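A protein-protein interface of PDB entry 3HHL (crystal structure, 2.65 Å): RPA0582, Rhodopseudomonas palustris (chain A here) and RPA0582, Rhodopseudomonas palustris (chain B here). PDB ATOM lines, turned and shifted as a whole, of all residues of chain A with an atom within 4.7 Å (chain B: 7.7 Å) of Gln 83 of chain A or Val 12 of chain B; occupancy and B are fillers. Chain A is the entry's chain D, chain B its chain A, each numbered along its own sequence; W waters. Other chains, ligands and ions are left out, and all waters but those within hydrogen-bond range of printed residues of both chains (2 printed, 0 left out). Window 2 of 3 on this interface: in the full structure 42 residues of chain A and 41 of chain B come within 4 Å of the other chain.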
ATOM      1  N   LEU A  77      15.284  -0.110  25.530  1.00  0.00           N
ATOM      2  CA  LEU A  77      14.845   0.851  26.533  1.00  0.00           C
ATOM      3  C   LEU A  77      13.380   1.181  26.402  1.00  0.00           C
ATOM      4  O   LEU A  77      12.857   1.341  25.278  1.00  0.00           O
ATOM      5  CB  LEU A  77      15.617   2.155  26.405  1.00  0.00           C
ATOM      6  CG  LEU A  77      15.610   3.088  27.615  1.00  0.00           C
ATOM      7  CD1 LEU A  77      16.500   2.495  28.663  1.00  0.00           C
ATOM      8  CD2 LEU A  77      16.070   4.519  27.264  1.00  0.00           C
ATOM      9  N   MET A  78      12.712   1.298  27.554  1.00  0.00           N
ATOM     10  CA  MET A  78      11.366   1.867  27.593  1.00  0.00           C
ATOM     11  C   MET A  78      11.581   3.371  27.793  1.00  0.00           C
ATOM     12  O   MET A  78      11.701   3.829  28.916  1.00  0.00           O
ATOM     13  CB  MET A  78      10.537   1.265  28.724  1.00  0.00           C
ATOM     14  CG  MET A  78       9.137   1.841  28.836  1.00  0.00           C
ATOM     15  SD  MET A  78       8.033   1.224  27.357  1.00  0.00           S
ATOM     16  CE  MET A  78       8.282  -0.686  27.486  1.00  0.00           C
ATOM     17  N   LEU A  79      11.670   4.118  26.693  1.00  0.00           N
ATOM     18  CA  LEU A  79      11.953   5.553  26.756  1.00  0.00           C
ATOM     19  C   LEU A  79      10.727   6.328  27.261  1.00  0.00           C
ATOM     20  O   LEU A  79      10.870   7.237  28.081  1.00  0.00           O
ATOM     21  CB  LEU A  79      12.398   6.085  25.398  1.00  0.00           C
ATOM     22  CG  LEU A  79      12.743   7.572  25.371  1.00  0.00           C
ATOM     23  CD1 LEU A  79      13.701   7.827  26.458  1.00  0.00           C
ATOM     24  CD2 LEU A  79      13.322   7.990  24.023  1.00  0.00           C
ATOM     25  N   GLY A  81       7.047   5.331  29.054  1.00  0.00           N
ATOM     26  CA  GLY A  81       6.301   4.235  29.636  1.00  0.00           C
ATOM     27  C   GLY A  81       6.863   3.942  30.990  1.00  0.00           C
ATOM     28  O   GLY A  81       7.835   4.580  31.397  1.00  0.00           O
ATOM     29  N   PRO A  82       6.280   2.972  31.701  1.00  0.00           N
ATOM     30  CA  PRO A  82       6.764   2.564  33.047  1.00  0.00           C
ATOM     31  C   PRO A  82       8.021   1.729  32.977  1.00  0.00           C
ATOM     32  O   PRO A  82       8.108   0.921  32.089  1.00  0.00           O
ATOM     33  CB  PRO A  82       5.629   1.699  33.559  1.00  0.00           C
ATOM     34  CG  PRO A  82       4.948   1.142  32.324  1.00  0.00           C
ATOM     35  CD  PRO A  82       5.177   2.128  31.209  1.00  0.00           C
ATOM     36  N   GLN A  83       8.972   1.863  33.893  1.00  0.00           N
ATOM     37  CA  GLN A  83      10.172   0.987  33.820  1.00  0.00           C
ATOM     38  C   GLN A  83       9.950  -0.498  34.161  1.00  0.00           C
ATOM     39  O   GLN A  83      10.731  -1.355  33.736  1.00  0.00           O
ATOM     40  CB  GLN A  83      11.336   1.540  34.629  1.00  0.00           C
ATOM     41  CG  GLN A  83      11.921   2.847  34.057  1.00  0.00           C
ATOM     42  CD  GLN A  83      12.310   2.808  32.529  1.00  0.00           C
ATOM     43  OE1 GLN A  83      13.354   2.268  32.139  1.00  0.00           O
ATOM     44  NE2 GLN A  83      11.497   3.447  31.703  1.00  0.00           N
ATOM     45  N   ASP A  84       8.887  -0.827  34.896  1.00  0.00           N
ATOM     46  CA  ASP A  84       8.588  -2.248  35.119  1.00  0.00           C
ATOM     47  C   ASP A  84       8.201  -2.963  33.804  1.00  0.00           C
ATOM     48  O   ASP A  84       8.130  -4.201  33.751  1.00  0.00           O
ATOM     49  CB  ASP A  84       7.538  -2.469  36.224  1.00  0.00           C
ATOM     50  CG  ASP A  84       6.216  -1.726  35.974  1.00  0.00           C
ATOM     51  OD1 ASP A  84       5.866  -0.878  36.822  1.00  0.00           O
ATOM     52  OD2 ASP A  84       5.504  -1.994  34.980  1.00  0.00           O
ATOM     53  N   GLU A  85       7.947  -2.203  32.743  1.00  0.00           N
ATOM     54  CA  GLU A  85       7.653  -2.817  31.453  1.00  0.00           C
ATOM     55  C   GLU A  85       8.949  -3.073  30.716  1.00  0.00           C
ATOM     56  O   GLU A  85       9.750  -2.182  30.527  1.00  0.00           O
ATOM     57  CB  GLU A  85       6.715  -1.972  30.606  1.00  0.00           C
ATOM     58  CG  GLU A  85       5.357  -2.575  30.501  1.00  0.00           C
ATOM     59  CD  GLU A  85       4.386  -1.715  29.753  1.00  0.00           C
ATOM     60  OE1 GLU A  85       4.735  -1.193  28.676  1.00  0.00           O
ATOM     61  OE2 GLU A  85       3.256  -1.555  30.255  1.00  0.00           O
ATOM     62  N   HIS B   5       1.441   7.596  30.387  1.00  0.00           N
ATOM     63  CA  HIS B   5       2.789   8.037  30.218  1.00  0.00           C
ATOM     64  C   HIS B   5       2.842   8.800  28.933  1.00  0.00           C
ATOM     65  O   HIS B   5       2.486   8.289  27.893  1.00  0.00           O
ATOM     66  CB  HIS B   5       3.713   6.833  30.165  1.00  0.00           C
ATOM     67  CG  HIS B   5       3.577   5.933  31.345  1.00  0.00           C
ATOM     68  ND1 HIS B   5       4.469   5.944  32.401  1.00  0.00           N
ATOM     69  CD2 HIS B   5       2.641   5.002  31.643  1.00  0.00           C
ATOM     70  CE1 HIS B   5       4.086   5.047  33.292  1.00  0.00           C
ATOM     71  NE2 HIS B   5       2.976   4.470  32.864  1.00  0.00           N
ATOM     72  N   ASP B   7       5.524  11.636  28.494  1.00  0.00           N
ATOM     73  CA  ASP B   7       6.885  12.089  28.248  1.00  0.00           C
ATOM     74  C   ASP B   7       7.910  11.180  28.894  1.00  0.00           C
ATOM     75  O   ASP B   7       7.614  10.442  29.787  1.00  0.00           O
ATOM     76  CB  ASP B   7       7.099  13.510  28.810  1.00  0.00           C
ATOM     77  CG  ASP B   7       6.418  14.606  27.978  1.00  0.00           C
ATOM     78  OD1 ASP B   7       6.485  14.603  26.721  1.00  0.00           O
ATOM     79  OD2 ASP B   7       5.825  15.488  28.623  1.00  0.00           O
ATOM     80  N   PRO B   8       9.136  11.230  28.409  1.00  0.00           N
ATOM     81  CA  PRO B   8      10.209  10.492  29.042  1.00  0.00           C
ATOM     82  C   PRO B   8      10.681  11.245  30.283  1.00  0.00           C
ATOM     83  O   PRO B   8      10.585  12.466  30.302  1.00  0.00           O
ATOM     84  CB  PRO B   8      11.272  10.492  27.975  1.00  0.00           C
ATOM     85  CG  PRO B   8      10.973  11.696  27.194  1.00  0.00           C
ATOM     86  CD  PRO B   8       9.545  11.848  27.152  1.00  0.00           C
ATOM     87  N   THR B   9      11.145  10.529  31.303  1.00  0.00           N
ATOM     88  CA  THR B   9      11.698  11.172  32.481  1.00  0.00           C
ATOM     89  C   THR B   9      13.178  11.520  32.198  1.00  0.00           C
ATOM     90  O   THR B   9      13.838  10.948  31.304  1.00  0.00           O
ATOM     91  CB  THR B   9      11.630  10.298  33.752  1.00  0.00           C
ATOM     92  OG1 THR B   9      12.618   9.270  33.675  1.00  0.00           O
ATOM     93  CG2 THR B   9      10.271   9.657  33.976  1.00  0.00           C
ATOM     94  N   LYS B  10      13.721  12.465  32.961  1.00  0.00           N
ATOM     95  CA  LYS B  10      15.093  12.881  32.677  1.00  0.00           C
ATOM     96  C   LYS B  10      16.132  11.744  32.883  1.00  0.00           C
ATOM     97  O   LYS B  10      17.128  11.664  32.175  1.00  0.00           O
ATOM     98  CB  LYS B  10      15.475  14.187  33.416  1.00  0.00           C
ATOM     99  CG  LYS B  10      15.314  14.202  34.946  1.00  0.00           C
ATOM    100  CD  LYS B  10      16.008  15.468  35.620  1.00  0.00           C
ATOM    101  CE  LYS B  10      15.393  15.891  36.979  1.00  0.00           C
ATOM    102  NZ  LYS B  10      15.166  14.756  37.909  1.00  0.00           N
ATOM    103  N   GLU B  11      15.863  10.872  33.838  1.00  0.00           N
ATOM    104  CA  GLU B  11      16.776   9.806  34.216  1.00  0.00           C
ATOM    105  C   GLU B  11      16.843   8.749  33.110  1.00  0.00           C
ATOM    106  O   GLU B  11      17.920   8.203  32.800  1.00  0.00           O
ATOM    107  CB  GLU B  11      16.323   9.147  35.516  1.00  0.00           C
ATOM    108  CG  GLU B  11      16.307  10.061  36.770  1.00  0.00           C
ATOM    109  CD  GLU B  11      15.022  10.986  36.896  1.00  0.00           C
ATOM    110  OE1 GLU B  11      13.849  10.570  36.558  1.00  0.00           O
ATOM    111  OE2 GLU B  11      15.199  12.157  37.358  1.00  0.00           O
ATOM    112  N   VAL B  12      15.687   8.454  32.520  1.00  0.00           N
ATOM    113  CA  VAL B  12      15.582   7.452  31.466  1.00  0.00           C
ATOM    114  C   VAL B  12      16.150   7.981  30.154  1.00  0.00           C
ATOM    115  O   VAL B  12      16.823   7.270  29.436  1.00  0.00           O
ATOM    116  CB  VAL B  12      14.133   6.991  31.333  1.00  0.00           C
ATOM    117  CG1 VAL B  12      13.905   6.128  30.032  1.00  0.00           C
ATOM    118  CG2 VAL B  12      13.742   6.236  32.594  1.00  0.00           C
ATOM    119  N   PHE B  13      15.928   9.249  29.859  1.00  0.00           N
ATOM    120  CA  PHE B  13      16.579   9.853  28.713  1.00  0.00           C
ATOM    121  C   PHE B  13      18.110   9.836  28.818  1.00  0.00           C
ATOM    122  O   PHE B  13      18.818   9.698  27.810  1.00  0.00           O
ATOM    123  CB  PHE B  13      16.079  11.277  28.494  1.00  0.00           C
ATOM    124  CG  PHE B  13      16.359  11.782  27.117  1.00  0.00           C
ATOM    125  CD1 PHE B  13      15.626  11.335  26.047  1.00  0.00           C
ATOM    126  CD2 PHE B  13      17.405  12.643  26.872  1.00  0.00           C
ATOM    127  CE1 PHE B  13      15.899  11.752  24.762  1.00  0.00           C
ATOM    128  CE2 PHE B  13      17.660  13.077  25.572  1.00  0.00           C
ATOM    129  CZ  PHE B  13      16.897  12.613  24.528  1.00  0.00           C
ATOM    130  N   ALA B  14      18.626   9.950  30.028  1.00  0.00           N
ATOM    131  CA  ALA B  14      20.060   9.844  30.240  1.00  0.00           C
ATOM    132  C   ALA B  14      20.535   8.441  29.842  1.00  0.00           C
ATOM    133  O   ALA B  14      21.532   8.284  29.157  1.00  0.00           O
ATOM    134  CB  ALA B  14      20.422  10.157  31.726  1.00  0.00           C
ATOM    135  N   GLN B  15      19.799   7.426  30.265  1.00  0.00           N
ATOM    136  CA  GLN B  15      20.102   6.072  29.909  1.00  0.00           C
ATOM    137  C   GLN B  15      20.093   5.863  28.377  1.00  0.00           C
ATOM    138  O   GLN B  15      20.884   5.079  27.856  1.00  0.00           O
ATOM    139  CB  GLN B  15      19.097   5.138  30.561  1.00  0.00           C
ATOM    140  CG  GLN B  15      19.320   4.945  32.066  1.00  0.00           C
ATOM    141  CD  GLN B  15      18.242   4.077  32.703  1.00  0.00           C
ATOM    142  OE1 GLN B  15      17.077   4.186  32.347  1.00  0.00           O
ATOM    143  NE2 GLN B  15      18.629   3.217  33.631  1.00  0.00           N
ATOM    144  N   PHE B  16      19.171   6.546  27.693  1.00  0.00           N
ATOM    145  CA  PHE B  16      19.040   6.462  26.254  1.00  0.00           C
ATOM    146  C   PHE B  16      20.303   6.979  25.601  1.00  0.00           C
ATOM    147  O   PHE B  16      20.875   6.311  24.750  1.00  0.00           O
ATOM    148  CB  PHE B  16      17.841   7.277  25.825  1.00  0.00           C
ATOM    149  CG  PHE B  16      17.631   7.369  24.333  1.00  0.00           C
ATOM    150  CD1 PHE B  16      16.883   6.425  23.668  1.00  0.00           C
ATOM    151  CD2 PHE B  16      18.087   8.470  23.623  1.00  0.00           C
ATOM    152  CE1 PHE B  16      16.649   6.522  22.290  1.00  0.00           C
ATOM    153  CE2 PHE B  16      17.876   8.576  22.265  1.00  0.00           C
ATOM    154  CZ  PHE B  16      17.141   7.589  21.592  1.00  0.00           C
ATOM    155  N   ARG B  17      20.738   8.169  26.011  1.00  0.00           N
ATOM    156  CA  ARG B  17      21.969   8.753  25.511  1.00  0.00           C
ATOM    157  C   ARG B  17      23.197   7.937  25.934  1.00  0.00           C
ATOM    158  O   ARG B  17      24.203   7.887  25.210  1.00  0.00           O
ATOM    159  CB  ARG B  17      22.123  10.184  26.036  1.00  0.00           C
ATOM    160  CG  ARG B  17      21.113  11.218  25.520  1.00  0.00           C
ATOM    161  CD  ARG B  17      21.374  12.596  26.151  1.00  0.00           C
ATOM    162  NE  ARG B  17      21.101  12.568  27.583  1.00  0.00           N
ATOM    163  CZ  ARG B  17      20.714  13.605  28.308  1.00  0.00           C
ATOM    164  NH1 ARG B  17      20.580  14.807  27.758  1.00  0.00           N
ATOM    165  NH2 ARG B  17      20.494  13.427  29.591  1.00  0.00           N
ATOM    166  N   ALA B  18      23.139   7.317  27.112  1.00  0.00           N
ATOM    167  CA  ALA B  18      24.295   6.529  27.606  1.00  0.00           C
ATOM    168  C   ALA B  18      24.593   5.363  26.642  1.00  0.00           C
ATOM    169  O   ALA B  18      25.751   5.057  26.368  1.00  0.00           O
ATOM    170  CB  ALA B  18      24.051   6.019  29.000  1.00  0.00           C
ATOM    171  N   LEU B 126       6.973   4.156  24.121  1.00  0.00           N
ATOM    172  CA  LEU B 126       8.001   4.420  23.115  1.00  0.00           C
ATOM    173  C   LEU B 126       9.133   3.514  23.474  1.00  0.00           C
ATOM    174  O   LEU B 126       9.844   3.760  24.446  1.00  0.00           O
ATOM    175  CB  LEU B 126       8.439   5.890  23.138  1.00  0.00           C
ATOM    176  CG  LEU B 126       9.413   6.365  22.056  1.00  0.00           C
ATOM    177  CD1 LEU B 126       8.796   6.189  20.750  1.00  0.00           C
ATOM    178  CD2 LEU B 126       9.789   7.819  22.253  1.00  0.00           C
HETATM  179  O   HOH W   1       7.860   7.954  30.464  1.00  0.00           O
HETATM  180  O   HOH W   2      10.638   7.532  30.833  1.00  0.00           O
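The backbone NH of Leu 79 of chain A is in hydrogen-bond range of the backbone carbonyl oxygen of Leu 126 of chain B, at 2.9 Å.
O of Met 78 of chain A lies within hydrogen-bond range of NE2 of Gln 83 of chain A, at 2.8 Å. The backbone NH (N) of Val 12 of chain B sits at hydrogen-bond distance from the side-chain hydroxyl (OG1) of Thr 9 of chain B.
Val 12 of chain B touches Leu 77 of chain A (O to CD2, 3.6 Å). Phe 16 of chain B touches Leu 77 of chain A. O of Leu 126 of chain B touches O of Leu 77 of chain A, at 3.95 Å. O of Met 78 of chain A touches CG1 of Val 12 of chain B, 3.4 Å away. O of Leu 126 of chain B touches C of Met 78 of chain A (3.8 Å). Leu 79 of chain A touches Val 12 of chain B (O to CG1, 3.8 Å). Phe 16 of chain B touches Leu 79 of chain A. C of Gly 81 of chain A touches ND1 of His 5 of chain B, 3.4 Å away. His 5 of chain B touches Pro 82 of chain A (CE1 to N, 3.4 Å). Gln 83 of chain A touches Val 12 of chain B.
Of the printed residues of chain B, Leu 79 of chain A touches Pro 8, Val 12, Phe 16 and Leu 126. Printed residues of chain B within 4 Å of Pro 82 of chain A: His 5. Of chain B, only Val 12 comes within 4 Å of Gln 83 of chain A. Of the printed residues of chain A, His 5 of chain B touches Gly 81 and Pro 82. Of chain A, only Leu 77, Met 78, Leu 79 and Gln 83 come within 4 Å of Val 12 of chain B. Ala 14 of chain B touches none of the printed residues of chain A. Of the printed residues of chain A, Phe 16 of chain B touches Leu 77 (3.6 Å) and Leu 79 (3.9 Å). Printed residues of chain A within 4 Å of Leu 126 of chain B: Leu 77 (3.95 Å), Met 78 (3.8 Å) and Leu 79 (2.9 Å).
Hydrophobic or aromatic side chains of chain A that line the printed part of chain B: Leu 77, Leu 79 and Pro 82. Printed residues of chain B that touch a printed residue of chain A: His 5, Pro 8, Val 12, Phe 16 and Leu 126. Among the printed residues, 12 pairs touch across the chains. Among the printed residues, no Asp or Glu carboxylate lies within 4 Å of a Lys or Arg side-chain nitrogen of the other chain.
Water W1 lies within hydrogen-bond range of the backbone carbonyl oxygen of Asp 7 of chain B (2.6 Å) and the backbone NH of Gly 81 of chain A (3.1 Å). Water W2 lies within hydrogen-bond range of the backbone carbonyl oxygen (O) of Leu 79 of chain A and the backbone NH (N) of Thr 9 of chain B.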
